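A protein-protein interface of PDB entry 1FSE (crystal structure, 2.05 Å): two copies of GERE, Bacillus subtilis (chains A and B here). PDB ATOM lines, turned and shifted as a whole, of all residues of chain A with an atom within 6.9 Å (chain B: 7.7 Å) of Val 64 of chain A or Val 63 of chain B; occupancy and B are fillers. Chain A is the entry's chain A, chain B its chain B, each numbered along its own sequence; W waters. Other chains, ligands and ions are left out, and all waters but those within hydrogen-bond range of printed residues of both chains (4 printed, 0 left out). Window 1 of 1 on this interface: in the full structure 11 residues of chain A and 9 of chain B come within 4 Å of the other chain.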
ATOM      1  N   ARG A  59     -26.441 -13.727  -9.366  1.00  0.00           N
ATOM      2  CA  ARG A  59     -26.537 -14.784 -10.373  1.00  0.00           C
ATOM      3  C   ARG A  59     -25.956 -14.324 -11.705  1.00  0.00           C
ATOM      4  O   ARG A  59     -25.247 -15.058 -12.386  1.00  0.00           O
ATOM      5  CB  ARG A  59     -28.007 -15.117 -10.602  1.00  0.00           C
ATOM      6  CG  ARG A  59     -28.579 -16.132  -9.630  1.00  0.00           C
ATOM      7  CD  ARG A  59     -30.098 -16.041  -9.625  1.00  0.00           C
ATOM      8  NE  ARG A  59     -30.641 -16.784  -8.492  1.00  0.00           N
ATOM      9  CZ  ARG A  59     -31.772 -17.482  -8.506  1.00  0.00           C
ATOM     10  NH1 ARG A  59     -32.510 -17.515  -9.614  1.00  0.00           N
ATOM     11  NH2 ARG A  59     -32.155 -18.124  -7.405  1.00  0.00           N
ATOM     12  N   SER A  60     -26.321 -13.109 -12.085  1.00  0.00           N
ATOM     13  CA  SER A  60     -25.842 -12.547 -13.333  1.00  0.00           C
ATOM     14  C   SER A  60     -24.330 -12.441 -13.300  1.00  0.00           C
ATOM     15  O   SER A  60     -23.703 -12.781 -14.290  1.00  0.00           O
ATOM     16  CB  SER A  60     -26.567 -11.255 -13.703  1.00  0.00           C
ATOM     17  OG  SER A  60     -25.977 -10.122 -13.106  1.00  0.00           O
ATOM     18  N   GLN A  61     -23.719 -12.038 -12.186  1.00  0.00           N
ATOM     19  CA  GLN A  61     -22.257 -11.980 -12.182  1.00  0.00           C
ATOM     20  C   GLN A  61     -21.659 -13.394 -12.354  1.00  0.00           C
ATOM     21  O   GLN A  61     -20.627 -13.523 -13.024  1.00  0.00           O
ATOM     22  CB  GLN A  61     -21.747 -11.250 -10.931  1.00  0.00           C
ATOM     23  CG  GLN A  61     -22.507  -9.936 -10.731  1.00  0.00           C
ATOM     24  CD  GLN A  61     -22.239  -9.163  -9.448  1.00  0.00           C
ATOM     25  OE1 GLN A  61     -23.001  -8.242  -9.121  1.00  0.00           O
ATOM     26  NE2 GLN A  61     -21.160  -9.493  -8.743  1.00  0.00           N
ATOM     27  N   ALA A  62     -22.304 -14.425 -11.797  1.00  0.00           N
ATOM     28  CA  ALA A  62     -21.814 -15.803 -11.883  1.00  0.00           C
ATOM     29  C   ALA A  62     -21.810 -16.298 -13.332  1.00  0.00           C
ATOM     30  O   ALA A  62     -20.822 -16.820 -13.850  1.00  0.00           O
ATOM     31  CB  ALA A  62     -22.609 -16.750 -11.012  1.00  0.00           C
ATOM     32  N   VAL A  63     -22.917 -16.013 -14.003  1.00  0.00           N
ATOM     33  CA  VAL A  63     -23.071 -16.282 -15.424  1.00  0.00           C
ATOM     34  C   VAL A  63     -22.013 -15.558 -16.236  1.00  0.00           C
ATOM     35  O   VAL A  63     -21.425 -16.144 -17.148  1.00  0.00           O
ATOM     36  CB  VAL A  63     -24.483 -15.897 -15.935  1.00  0.00           C
ATOM     37  CG1 VAL A  63     -24.554 -15.947 -17.463  1.00  0.00           C
ATOM     38  CG2 VAL A  63     -25.552 -16.789 -15.304  1.00  0.00           C
ATOM     39  N   VAL A  64     -21.786 -14.280 -15.962  1.00  0.00           N
ATOM     40  CA  VAL A  64     -20.767 -13.569 -16.723  1.00  0.00           C
ATOM     41  C   VAL A  64     -19.390 -14.174 -16.442  1.00  0.00           C
ATOM     42  O   VAL A  64     -18.644 -14.387 -17.392  1.00  0.00           O
ATOM     43  CB  VAL A  64     -20.761 -12.046 -16.437  1.00  0.00           C
ATOM     44  CG1 VAL A  64     -19.524 -11.354 -17.003  1.00  0.00           C
ATOM     45  CG2 VAL A  64     -22.006 -11.355 -17.010  1.00  0.00           C
ATOM     46  N   GLU A  65     -19.051 -14.515 -15.198  1.00  0.00           N
ATOM     47  CA  GLU A  65     -17.720 -15.080 -14.961  1.00  0.00           C
ATOM     48  C   GLU A  65     -17.560 -16.456 -15.613  1.00  0.00           C
ATOM     49  O   GLU A  65     -16.512 -16.744 -16.173  1.00  0.00           O
ATOM     50  CB  GLU A  65     -17.341 -15.231 -13.484  1.00  0.00           C
ATOM     51  CG  GLU A  65     -17.298 -13.942 -12.691  1.00  0.00           C
ATOM     52  CD  GLU A  65     -16.126 -13.048 -13.059  1.00  0.00           C
ATOM     53  OE1 GLU A  65     -15.080 -13.578 -13.499  1.00  0.00           O
ATOM     54  OE2 GLU A  65     -16.262 -11.816 -12.880  1.00  0.00           O
ATOM     55  N   LEU A  66     -18.588 -17.295 -15.566  1.00  0.00           N
ATOM     56  CA  LEU A  66     -18.528 -18.573 -16.252  1.00  0.00           C
ATOM     57  C   LEU A  66     -18.412 -18.417 -17.776  1.00  0.00           C
ATOM     58  O   LEU A  66     -17.805 -19.264 -18.444  1.00  0.00           O
ATOM     59  CB  LEU A  66     -19.716 -19.464 -15.878  1.00  0.00           C
ATOM     60  CG  LEU A  66     -19.734 -19.980 -14.430  1.00  0.00           C
ATOM     61  CD1 LEU A  66     -21.126 -20.498 -14.125  1.00  0.00           C
ATOM     62  CD2 LEU A  66     -18.633 -21.009 -14.211  1.00  0.00           C
ATOM     63  N   LEU A  67     -19.008 -17.380 -18.357  1.00  0.00           N
ATOM     64  CA  LEU A  67     -18.877 -17.156 -19.796  1.00  0.00           C
ATOM     65  C   LEU A  67     -17.429 -16.802 -20.093  1.00  0.00           C
ATOM     66  O   LEU A  67     -16.824 -17.294 -21.048  1.00  0.00           O
ATOM     67  CB  LEU A  67     -19.785 -16.032 -20.304  1.00  0.00           C
ATOM     68  CG  LEU A  67     -21.236 -16.516 -20.344  1.00  0.00           C
ATOM     69  CD1 LEU A  67     -22.145 -15.359 -20.754  1.00  0.00           C
ATOM     70  CD2 LEU A  67     -21.349 -17.727 -21.269  1.00  0.00           C
ATOM     71  N   ARG A  68     -16.871 -15.958 -19.238  1.00  0.00           N
ATOM     72  CA  ARG A  68     -15.484 -15.547 -19.397  1.00  0.00           C
ATOM     73  C   ARG A  68     -14.486 -16.696 -19.404  1.00  0.00           C
ATOM     74  O   ARG A  68     -13.589 -16.720 -20.234  1.00  0.00           O
ATOM     75  CB  ARG A  68     -15.108 -14.569 -18.294  1.00  0.00           C
ATOM     76  CG  ARG A  68     -15.537 -13.169 -18.647  1.00  0.00           C
ATOM     77  CD  ARG A  68     -15.359 -12.152 -17.543  1.00  0.00           C
ATOM     78  NE  ARG A  68     -15.930 -10.907 -18.040  1.00  0.00           N
ATOM     79  CZ  ARG A  68     -16.129  -9.843 -17.284  1.00  0.00           C
ATOM     80  NH1 ARG A  68     -15.748  -9.915 -16.014  1.00  0.00           N
ATOM     81  NH2 ARG A  68     -16.663  -8.738 -17.794  1.00  0.00           N
ATOM     82  N   MET A  69     -14.627 -17.598 -18.438  1.00  0.00           N
ATOM     83  CA  MET A  69     -13.821 -18.804 -18.292  1.00  0.00           C
ATOM     84  C   MET A  69     -14.099 -19.920 -19.300  1.00  0.00           C
ATOM     85  O   MET A  69     -13.436 -20.958 -19.279  1.00  0.00           O
ATOM     86  CB  MET A  69     -14.174 -19.444 -16.950  1.00  0.00           C
ATOM     87  CG  MET A  69     -13.709 -18.738 -15.692  1.00  0.00           C
ATOM     88  SD  MET A  69     -14.632 -19.349 -14.232  1.00  0.00           S
ATOM     89  CE  MET A  69     -13.897 -18.180 -13.157  1.00  0.00           C
ATOM     90  N   LEU A  72     -19.520 -21.934 -19.774  1.00  0.00           N
ATOM     91  CA  LEU A  72     -20.886 -21.848 -20.264  1.00  0.00           C
ATOM     92  C   LEU A  72     -20.829 -21.423 -21.724  1.00  0.00           C
ATOM     93  O   LEU A  72     -19.903 -20.721 -22.149  1.00  0.00           O
ATOM     94  CB  LEU A  72     -21.693 -20.814 -19.479  1.00  0.00           C
ATOM     95  CG  LEU A  72     -22.548 -21.203 -18.273  1.00  0.00           C
ATOM     96  CD1 LEU A  72     -23.423 -20.025 -17.848  1.00  0.00           C
ATOM     97  CD2 LEU A  72     -23.390 -22.431 -18.638  1.00  0.00           C
ATOM     98  N   LEU A  74     -23.597 -19.871 -24.769  1.00  0.00           N
ATOM     99  CA  LEU A  74     -24.897 -19.350 -25.165  1.00  0.00           C
ATOM    100  C   LEU A  74     -25.127 -19.845 -26.591  1.00  0.00           C
ATOM    101  O   LEU A  74     -26.238 -19.817 -27.125  1.00  0.00           O
ATOM    102  CB  LEU A  74     -24.847 -17.823 -25.147  1.00  0.00           C
ATOM    103  CG  LEU A  74     -24.421 -17.232 -23.801  1.00  0.00           C
ATOM    104  CD1 LEU A  74     -24.654 -15.745 -23.833  1.00  0.00           C
ATOM    105  CD2 LEU A  74     -25.218 -17.841 -22.657  1.00  0.00           C
ATOM    106  N   PHE B  20     -25.803  -1.587 -18.101  1.00  0.00           N
ATOM    107  CA  PHE B  20     -25.546  -3.016 -18.248  1.00  0.00           C
ATOM    108  C   PHE B  20     -24.055  -3.345 -18.367  1.00  0.00           C
ATOM    109  O   PHE B  20     -23.578  -4.340 -17.801  1.00  0.00           O
ATOM    110  CB  PHE B  20     -26.386  -3.632 -19.372  1.00  0.00           C
ATOM    111  CG  PHE B  20     -27.717  -4.116 -18.907  1.00  0.00           C
ATOM    112  CD1 PHE B  20     -27.844  -5.391 -18.385  1.00  0.00           C
ATOM    113  CD2 PHE B  20     -28.825  -3.291 -18.964  1.00  0.00           C
ATOM    114  CE1 PHE B  20     -29.054  -5.829 -17.901  1.00  0.00           C
ATOM    115  CE2 PHE B  20     -30.048  -3.741 -18.500  1.00  0.00           C
ATOM    116  CZ  PHE B  20     -30.156  -5.002 -17.963  1.00  0.00           C
ATOM    117  N   LEU B  23     -22.890  -3.274 -14.837  1.00  0.00           N
ATOM    118  CA  LEU B  23     -23.450  -4.500 -14.274  1.00  0.00           C
ATOM    119  C   LEU B  23     -22.584  -5.746 -14.495  1.00  0.00           C
ATOM    120  O   LEU B  23     -22.312  -6.457 -13.530  1.00  0.00           O
ATOM    121  CB  LEU B  23     -24.852  -4.723 -14.835  1.00  0.00           C
ATOM    122  CG  LEU B  23     -25.945  -4.993 -13.807  1.00  0.00           C
ATOM    123  CD1 LEU B  23     -25.688  -4.175 -12.554  1.00  0.00           C
ATOM    124  CD2 LEU B  23     -27.361  -4.779 -14.308  1.00  0.00           C
ATOM    125  N   VAL B  24     -22.077  -5.943 -15.705  1.00  0.00           N
ATOM    126  CA  VAL B  24     -21.216  -7.080 -16.042  1.00  0.00           C
ATOM    127  C   VAL B  24     -19.766  -6.936 -15.552  1.00  0.00           C
ATOM    128  O   VAL B  24     -18.939  -7.840 -15.704  1.00  0.00           O
ATOM    129  CB  VAL B  24     -21.279  -7.439 -17.538  1.00  0.00           C
ATOM    130  CG1 VAL B  24     -22.704  -7.786 -17.922  1.00  0.00           C
ATOM    131  CG2 VAL B  24     -20.779  -6.310 -18.434  1.00  0.00           C
ATOM    132  N   GLN B  25     -19.476  -5.835 -14.867  1.00  0.00           N
ATOM    133  CA  GLN B  25     -18.128  -5.648 -14.330  1.00  0.00           C
ATOM    134  C   GLN B  25     -18.254  -5.823 -12.836  1.00  0.00           C
ATOM    135  O   GLN B  25     -17.373  -5.400 -12.097  1.00  0.00           O
ATOM    136  CB  GLN B  25     -17.553  -4.247 -14.548  1.00  0.00           C
ATOM    137  CG  GLN B  25     -17.083  -3.973 -15.953  1.00  0.00           C
ATOM    138  CD  GLN B  25     -16.773  -2.503 -16.225  1.00  0.00           C
ATOM    139  OE1 GLN B  25     -16.829  -2.072 -17.378  1.00  0.00           O
ATOM    140  NE2 GLN B  25     -16.507  -1.725 -15.185  1.00  0.00           N
ATOM    141  N   ASP B  26     -19.398  -6.344 -12.406  1.00  0.00           N
ATOM    142  CA  ASP B  26     -19.607  -6.637 -11.000  1.00  0.00           C
ATOM    143  C   ASP B  26     -19.963  -5.472 -10.097  1.00  0.00           C
ATOM    144  O   ASP B  26     -19.844  -5.584  -8.875  1.00  0.00           O
ATOM    145  CB  ASP B  26     -18.339  -7.220 -10.387  1.00  0.00           C
ATOM    146  CG  ASP B  26     -18.544  -8.637  -9.997  1.00  0.00           C
ATOM    147  OD1 ASP B  26     -18.740  -9.395 -10.985  1.00  0.00           O
ATOM    148  OD2 ASP B  26     -18.525  -8.995  -8.785  1.00  0.00           O
ATOM    149  N   MET B  51     -35.372  -4.988 -19.060  1.00  0.00           N
ATOM    150  CA  MET B  51     -35.853  -6.362 -19.000  1.00  0.00           C
ATOM    151  C   MET B  51     -37.295  -6.475 -19.501  1.00  0.00           C
ATOM    152  O   MET B  51     -37.716  -7.491 -20.038  1.00  0.00           O
ATOM    153  CB  MET B  51     -35.769  -6.834 -17.548  1.00  0.00           C
ATOM    154  CG  MET B  51     -34.336  -7.163 -17.122  1.00  0.00           C
ATOM    155  SD  MET B  51     -34.148  -7.202 -15.335  1.00  0.00           S
ATOM    156  CE  MET B  51     -35.768  -7.874 -14.931  1.00  0.00           C
ATOM    157  N   LEU B  54     -36.961  -6.863 -23.226  1.00  0.00           N
ATOM    158  CA  LEU B  54     -36.536  -8.192 -23.655  1.00  0.00           C
ATOM    159  C   LEU B  54     -37.568  -9.271 -23.324  1.00  0.00           C
ATOM    160  O   LEU B  54     -37.546 -10.382 -23.854  1.00  0.00           O
ATOM    161  CB  LEU B  54     -35.204  -8.526 -22.978  1.00  0.00           C
ATOM    162  CG  LEU B  54     -34.023  -7.630 -23.333  1.00  0.00           C
ATOM    163  CD1 LEU B  54     -33.015  -7.782 -22.225  1.00  0.00           C
ATOM    164  CD2 LEU B  54     -33.402  -8.144 -24.612  1.00  0.00           C
ATOM    165  N   VAL B  56     -37.971 -10.634 -20.303  1.00  0.00           N
ATOM    166  CA  VAL B  56     -37.392 -11.616 -19.392  1.00  0.00           C
ATOM    167  C   VAL B  56     -37.585 -11.172 -17.948  1.00  0.00           C
ATOM    168  O   VAL B  56     -37.666  -9.972 -17.687  1.00  0.00           O
ATOM    169  CB  VAL B  56     -35.898 -11.824 -19.666  1.00  0.00           C
ATOM    170  CG1 VAL B  56     -35.765 -12.504 -21.011  1.00  0.00           C
ATOM    171  CG2 VAL B  56     -35.132 -10.481 -19.589  1.00  0.00           C
ATOM    172  N   GLY B  58     -35.468 -12.028 -15.252  1.00  0.00           N
ATOM    173  CA  GLY B  58     -34.302 -11.849 -14.408  1.00  0.00           C
ATOM    174  C   GLY B  58     -33.135 -11.157 -15.076  1.00  0.00           C
ATOM    175  O   GLY B  58     -33.093 -11.041 -16.303  1.00  0.00           O
ATOM    176  N   ARG B  59     -32.227 -10.642 -14.254  1.00  0.00           N
ATOM    177  CA  ARG B  59     -31.062  -9.944 -14.780  1.00  0.00           C
ATOM    178  C   ARG B  59     -30.143 -10.879 -15.551  1.00  0.00           C
ATOM    179  O   ARG B  59     -29.575 -10.436 -16.538  1.00  0.00           O
ATOM    180  CB  ARG B  59     -30.224  -9.386 -13.632  1.00  0.00           C
ATOM    181  CG  ARG B  59     -30.567  -7.999 -13.176  1.00  0.00           C
ATOM    182  CD  ARG B  59     -29.660  -7.640 -12.020  1.00  0.00           C
ATOM    183  NE  ARG B  59     -30.255  -6.577 -11.221  1.00  0.00           N
ATOM    184  CZ  ARG B  59     -29.525  -5.866 -10.383  1.00  0.00           C
ATOM    185  NH1 ARG B  59     -28.230  -6.156 -10.278  1.00  0.00           N
ATOM    186  NH2 ARG B  59     -30.096  -4.879  -9.700  1.00  0.00           N
ATOM    187  N   SER B  60     -29.934 -12.097 -15.055  1.00  0.00           N
ATOM    188  CA  SER B  60     -29.134 -13.107 -15.744  1.00  0.00           C
ATOM    189  C   SER B  60     -29.602 -13.280 -17.183  1.00  0.00           C
ATOM    190  O   SER B  60     -28.757 -13.343 -18.078  1.00  0.00           O
ATOM    191  CB  SER B  60     -29.194 -14.508 -15.131  1.00  0.00           C
ATOM    192  OG  SER B  60     -28.549 -14.626 -13.872  1.00  0.00           O
ATOM    193  N   GLN B  61     -30.909 -13.472 -17.364  1.00  0.00           N
ATOM    194  CA  GLN B  61     -31.478 -13.666 -18.693  1.00  0.00           C
ATOM    195  C   GLN B  61     -31.393 -12.370 -19.502  1.00  0.00           C
ATOM    196  O   GLN B  61     -31.198 -12.445 -20.706  1.00  0.00           O
ATOM    197  CB  GLN B  61     -32.875 -14.309 -18.744  1.00  0.00           C
ATOM    198  CG  GLN B  61     -33.854 -14.049 -17.627  1.00  0.00           C
ATOM    199  CD  GLN B  61     -35.066 -14.960 -17.669  1.00  0.00           C
ATOM    200  OE1 GLN B  61     -35.461 -15.504 -16.640  1.00  0.00           O
ATOM    201  NE2 GLN B  61     -35.648 -15.147 -18.850  1.00  0.00           N
ATOM    202  N   ALA B  62     -31.443 -11.198 -18.876  1.00  0.00           N
ATOM    203  CA  ALA B  62     -31.294  -9.981 -19.663  1.00  0.00           C
ATOM    204  C   ALA B  62     -29.889  -9.916 -20.241  1.00  0.00           C
ATOM    205  O   ALA B  62     -29.744  -9.644 -21.434  1.00  0.00           O
ATOM    206  CB  ALA B  62     -31.649  -8.719 -18.884  1.00  0.00           C
ATOM    207  N   VAL B  63     -28.892 -10.257 -19.422  1.00  0.00           N
ATOM    208  CA  VAL B  63     -27.489 -10.231 -19.822  1.00  0.00           C
ATOM    209  C   VAL B  63     -27.224 -11.210 -20.970  1.00  0.00           C
ATOM    210  O   VAL B  63     -26.579 -10.908 -21.979  1.00  0.00           O
ATOM    211  CB  VAL B  63     -26.615 -10.564 -18.601  1.00  0.00           C
ATOM    212  CG1 VAL B  63     -25.169 -10.824 -18.999  1.00  0.00           C
ATOM    213  CG2 VAL B  63     -26.674  -9.436 -17.580  1.00  0.00           C
ATOM    214  N   VAL B  64     -27.730 -12.424 -20.794  1.00  0.00           N
ATOM    215  CA  VAL B  64     -27.544 -13.444 -21.814  1.00  0.00           C
ATOM    216  C   VAL B  64     -28.172 -12.998 -23.130  1.00  0.00           C
ATOM    217  O   VAL B  64     -27.518 -13.111 -24.161  1.00  0.00           O
ATOM    218  CB  VAL B  64     -28.169 -14.781 -21.361  1.00  0.00           C
ATOM    219  CG1 VAL B  64     -28.293 -15.752 -22.525  1.00  0.00           C
ATOM    220  CG2 VAL B  64     -27.323 -15.362 -20.231  1.00  0.00           C
ATOM    221  N   GLU B  65     -29.414 -12.516 -23.099  1.00  0.00           N
ATOM    222  CA  GLU B  65     -30.112 -12.118 -24.319  1.00  0.00           C
ATOM    223  C   GLU B  65     -29.443 -10.923 -24.983  1.00  0.00           C
ATOM    224  O   GLU B  65     -29.208 -10.936 -26.190  1.00  0.00           O
ATOM    225  CB  GLU B  65     -31.602 -11.856 -24.098  1.00  0.00           C
ATOM    226  CG  GLU B  65     -32.425 -13.047 -23.623  1.00  0.00           C
ATOM    227  CD  GLU B  65     -32.114 -14.405 -24.243  1.00  0.00           C
ATOM    228  OE1 GLU B  65     -30.966 -14.646 -24.689  1.00  0.00           O
ATOM    229  OE2 GLU B  65     -32.991 -15.306 -24.194  1.00  0.00           O
ATOM    230  N   LEU B  66     -29.070  -9.938 -24.167  1.00  0.00           N
ATOM    231  CA  LEU B  66     -28.346  -8.783 -24.682  1.00  0.00           C
ATOM    232  C   LEU B  66     -27.049  -9.225 -25.355  1.00  0.00           C
ATOM    233  O   LEU B  66     -26.703  -8.680 -26.407  1.00  0.00           O
ATOM    234  CB  LEU B  66     -28.109  -7.681 -23.635  1.00  0.00           C
ATOM    235  CG  LEU B  66     -29.366  -7.013 -23.053  1.00  0.00           C
ATOM    236  CD1 LEU B  66     -29.073  -6.221 -21.777  1.00  0.00           C
ATOM    237  CD2 LEU B  66     -30.129  -6.152 -24.074  1.00  0.00           C
ATOM    238  N   LEU B  67     -26.364 -10.208 -24.778  1.00  0.00           N
ATOM    239  CA  LEU B  67     -25.124 -10.720 -25.347  1.00  0.00           C
ATOM    240  C   LEU B  67     -25.433 -11.419 -26.667  1.00  0.00           C
ATOM    241  O   LEU B  67     -24.648 -11.326 -27.612  1.00  0.00           O
ATOM    242  CB  LEU B  67     -24.406 -11.694 -24.411  1.00  0.00           C
ATOM    243  CG  LEU B  67     -23.618 -11.172 -23.201  1.00  0.00           C
ATOM    244  CD1 LEU B  67     -23.103 -12.370 -22.412  1.00  0.00           C
ATOM    245  CD2 LEU B  67     -22.426 -10.329 -23.635  1.00  0.00           C
ATOM    246  N   ARG B  68     -26.575 -12.096 -26.747  1.00  0.00           N
ATOM    247  CA  ARG B  68     -26.899 -12.818 -27.967  1.00  0.00           C
ATOM    248  C   ARG B  68     -27.215 -11.834 -29.075  1.00  0.00           C
ATOM    249  O   ARG B  68     -26.859 -12.069 -30.228  1.00  0.00           O
ATOM    250  CB  ARG B  68     -28.090 -13.763 -27.783  1.00  0.00           C
ATOM    251  CG  ARG B  68     -27.688 -15.076 -27.135  1.00  0.00           C
ATOM    252  CD  ARG B  68     -28.832 -16.060 -27.017  1.00  0.00           C
ATOM    253  NE  ARG B  68     -28.373 -17.424 -26.788  1.00  0.00           N
ATOM    254  CZ  ARG B  68     -28.969 -18.193 -25.896  1.00  0.00           C
ATOM    255  NH1 ARG B  68     -29.991 -17.653 -25.247  1.00  0.00           N
ATOM    256  NH2 ARG B  68     -28.585 -19.446 -25.683  1.00  0.00           N
ATOM    257  N   MET B  69     -27.868 -10.743 -28.684  1.00  0.00           N
ATOM    258  CA  MET B  69     -28.280  -9.691 -29.603  1.00  0.00           C
ATOM    259  C   MET B  69     -27.174  -8.748 -30.044  1.00  0.00           C
ATOM    260  O   MET B  69     -27.449  -7.945 -30.917  1.00  0.00           O
ATOM    261  CB  MET B  69     -29.440  -8.870 -29.021  1.00  0.00           C
ATOM    262  CG  MET B  69     -30.739  -9.682 -28.910  1.00  0.00           C
ATOM    263  SD  MET B  69     -31.936  -8.914 -27.791  1.00  0.00           S
ATOM    264  CE  MET B  69     -32.059  -7.413 -28.705  1.00  0.00           C
ATOM    265  N   GLU B  71     -25.963  -6.373 -28.185  1.00  0.00           N
ATOM    266  CA  GLU B  71     -26.278  -5.076 -27.595  1.00  0.00           C
ATOM    267  C   GLU B  71     -25.416  -4.805 -26.376  1.00  0.00           C
ATOM    268  O   GLU B  71     -25.608  -3.785 -25.718  1.00  0.00           O
ATOM    269  CB  GLU B  71     -27.716  -5.036 -27.072  1.00  0.00           C
ATOM    270  CG  GLU B  71     -28.839  -5.238 -28.085  1.00  0.00           C
ATOM    271  CD  GLU B  71     -29.509  -3.917 -28.435  1.00  0.00           C
ATOM    272  OE1 GLU B  71     -29.262  -2.923 -27.713  1.00  0.00           O
ATOM    273  OE2 GLU B  71     -30.245  -3.864 -29.446  1.00  0.00           O
ATOM    274  N   LEU B  72     -24.505  -5.712 -26.047  1.00  0.00           N
ATOM    275  CA  LEU B  72     -23.692  -5.629 -24.840  1.00  0.00           C
ATOM    276  C   LEU B  72     -22.476  -6.487 -25.159  1.00  0.00           C
ATOM    277  O   LEU B  72     -22.589  -7.532 -25.810  1.00  0.00           O
ATOM    278  CB  LEU B  72     -24.454  -6.255 -23.672  1.00  0.00           C
ATOM    279  CG  LEU B  72     -23.928  -6.146 -22.242  1.00  0.00           C
ATOM    280  CD1 LEU B  72     -23.868  -4.653 -21.958  1.00  0.00           C
ATOM    281  CD2 LEU B  72     -24.899  -6.787 -21.271  1.00  0.00           C
ATOM    282  N   GLU B  73     -21.322  -6.086 -24.646  1.00  0.00           N
ATOM    283  CA  GLU B  73     -20.108  -6.784 -25.054  1.00  0.00           C
ATOM    284  C   GLU B  73     -19.309  -7.731 -24.157  1.00  0.00           C
ATOM    285  O   GLU B  73     -18.932  -8.814 -24.604  1.00  0.00           O
ATOM    286  CB  GLU B  73     -19.157  -5.803 -25.743  1.00  0.00           C
ATOM    287  CG  GLU B  73     -18.999  -6.108 -27.231  1.00  0.00           C
ATOM    288  CD  GLU B  73     -17.544  -6.333 -27.614  1.00  0.00           C
ATOM    289  OE1 GLU B  73     -16.739  -5.373 -27.592  1.00  0.00           O
ATOM    290  OE2 GLU B  73     -17.172  -7.497 -27.864  1.00  0.00           O
ATOM    291  N   LEU B  74     -18.970  -7.344 -22.937  1.00  0.00           N
ATOM    292  CA  LEU B  74     -18.092  -8.141 -22.077  1.00  0.00           C
ATOM    293  C   LEU B  74     -16.606  -7.893 -22.350  1.00  0.00           C
ATOM    294  O   LEU B  74     -16.126  -6.780 -22.138  1.00  0.00           O
ATOM    295  CB  LEU B  74     -18.378  -9.638 -22.143  1.00  0.00           C
ATOM    296  CG  LEU B  74     -19.042 -10.437 -21.025  1.00  0.00           C
ATOM    297  CD1 LEU B  74     -20.357  -9.832 -20.538  1.00  0.00           C
ATOM    298  CD2 LEU B  74     -19.209 -11.893 -21.419  1.00  0.00           C
HETATM  299  O   HOH W   1     -23.319  -6.522 -10.916  1.00  0.00           O
HETATM  300  O   HOH W   2     -16.112 -10.321 -10.056  1.00  0.00           O
HETATM  301  O   HOH W   3     -16.621  -6.041 -19.068  1.00  0.00           O
HETATM  302  O   HOH W   4     -23.404  -9.240 -13.888  1.00  0.00           O
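The backbone NH (N) of Ser 60 of chain A sits at hydrogen-bond distance from the side-chain hydroxyl (OG) of Ser 60 of chain B (3.2 Å).
The guanidinium group of Arg 68 of chain B sits at hydrogen-bond distance from the backbone carbonyl oxygen of Leu 74 of chain A.
O of Val 24 of chain B sits at hydrogen-bond distance from NH2 of Arg 68 of chain A (3.2 Å).
NE2 of Gln 61 of chain A is in hydrogen-bond range of OD2 of Asp 26 of chain B (2.7 Å).
Printed residues of chain B that touch a printed residue of chain A: Val 24, Asp 26, Ser 60, Val 63, Val 64, Leu 67, Arg 68 and Leu 74.
Hydrophobic or aromatic side chains of chain B within 4 Å of the printed part of chain A: Val 24, Val 63, Val 64, Leu 67 and Leu 74.
Arg 59 of chain A touches Ser 60 of chain B.
Val 63 of chain A touches Ser 60 of chain B (CG2 to OG, 3.96 Å).
Val 63 of chain A touches Val 64 of chain B (CG1 to CG2, 3.96 Å).
Val 24 of chain B touches Val 64 of chain A (CG1 to CG2, 3.7 Å).
CG2 of Val 64 of chain A touches CG1 of Val 63 of chain B (3.8 Å).
Val 64 of chain A touches Leu 74 of chain B (CG1 to CD1, 3.9 Å).
Glu 65 of chain A touches Asp 26 of chain B.
Leu 67 of chain A touches Leu 67 of chain B (CD1 to CD1, 3.5 Å).
Leu 74 of chain A touches Val 64 of chain B (CD2 to CG1, 3.7 Å).
Leu 74 of chain A touches Leu 67 of chain B (CD1 to CD1, 3.98 Å).
The side-chain carboxylate (OE1) of Glu 65 of chain B is in salt-bridge range of the guanidinium group (NH1) of Arg 68 of chain B (3.2 Å).
OE2 of Glu 65 of chain A lies within salt-bridge range of NH1 of Arg 68 of chain A (3.7 Å).
Arg 59 of chain A touches Ser 60 of chain B, but with the chains exchanged Ser 60 of chain A does not touch Arg 59 of chain B (4.04 Å).
Val 63 of chain A touches Ser 60 of chain B, but with the chains exchanged Ser 60 of chain A does not touch Val 63 of chain B (4.3 Å).
Leu 67 of chain A touches its own counterpart, Leu 67 of chain B.
Leu 74 of chain A touches Arg 68 of chain B, but with the chains exchanged Arg 68 of chain A does not touch Leu 74 of chain B (4.3 Å).
Positions printed for both chains: 59, 60, 61, 62, 63, 64, 65, 66, 67, 68, 69, 72 and 74.
Of the 14 pairs that touch across the chains among the printed residues, 6 have their exchanged pair printed and touching as well.
Water W1 bridges the side-chain amide oxygen (OE1) of Gln 61 of chain A (2.5 Å) and the backbone carbonyl oxygen (O) of Leu 23 of chain B (2.8 Å).
Water W4 lies within hydrogen-bond range of the side-chain hydroxyl of Ser 60 of chain A (2.8 Å), the backbone carbonyl oxygen of Leu 23 of chain B (3.0 Å) and the backbone NH of Gln 61 of chain A (3.3 Å).
Water W2 bridges OD1 of Asp 26 of chain B (2.9 Å) and OE2 of Glu 65 of chain A (3.2 Å).
Water W3 lies within hydrogen-bond range of NH2 of Arg 68 of chain A (3.0 Å) and O of Leu 74 of chain B (3.2 Å).
Of chain B, only Val 24, Val 63 and Leu 74 come within 4 Å of Val 64 of chain A.
Of the printed residues of chain B, Leu 67 of chain A touches Leu 67.
Leu 72 of chain A touches none of the printed residues of chain B.
Of the printed residues of chain B, Leu 74 of chain A touches Val 64 (3.7 Å), Leu 67 (3.98 Å) and Arg 68 (2.8 Å).
Val 63 of chain B touches one residue of chain A.
The nearest residue of chain B that does not touch Val 64 of chain A is Leu 67 of chain B (5.6 Å).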
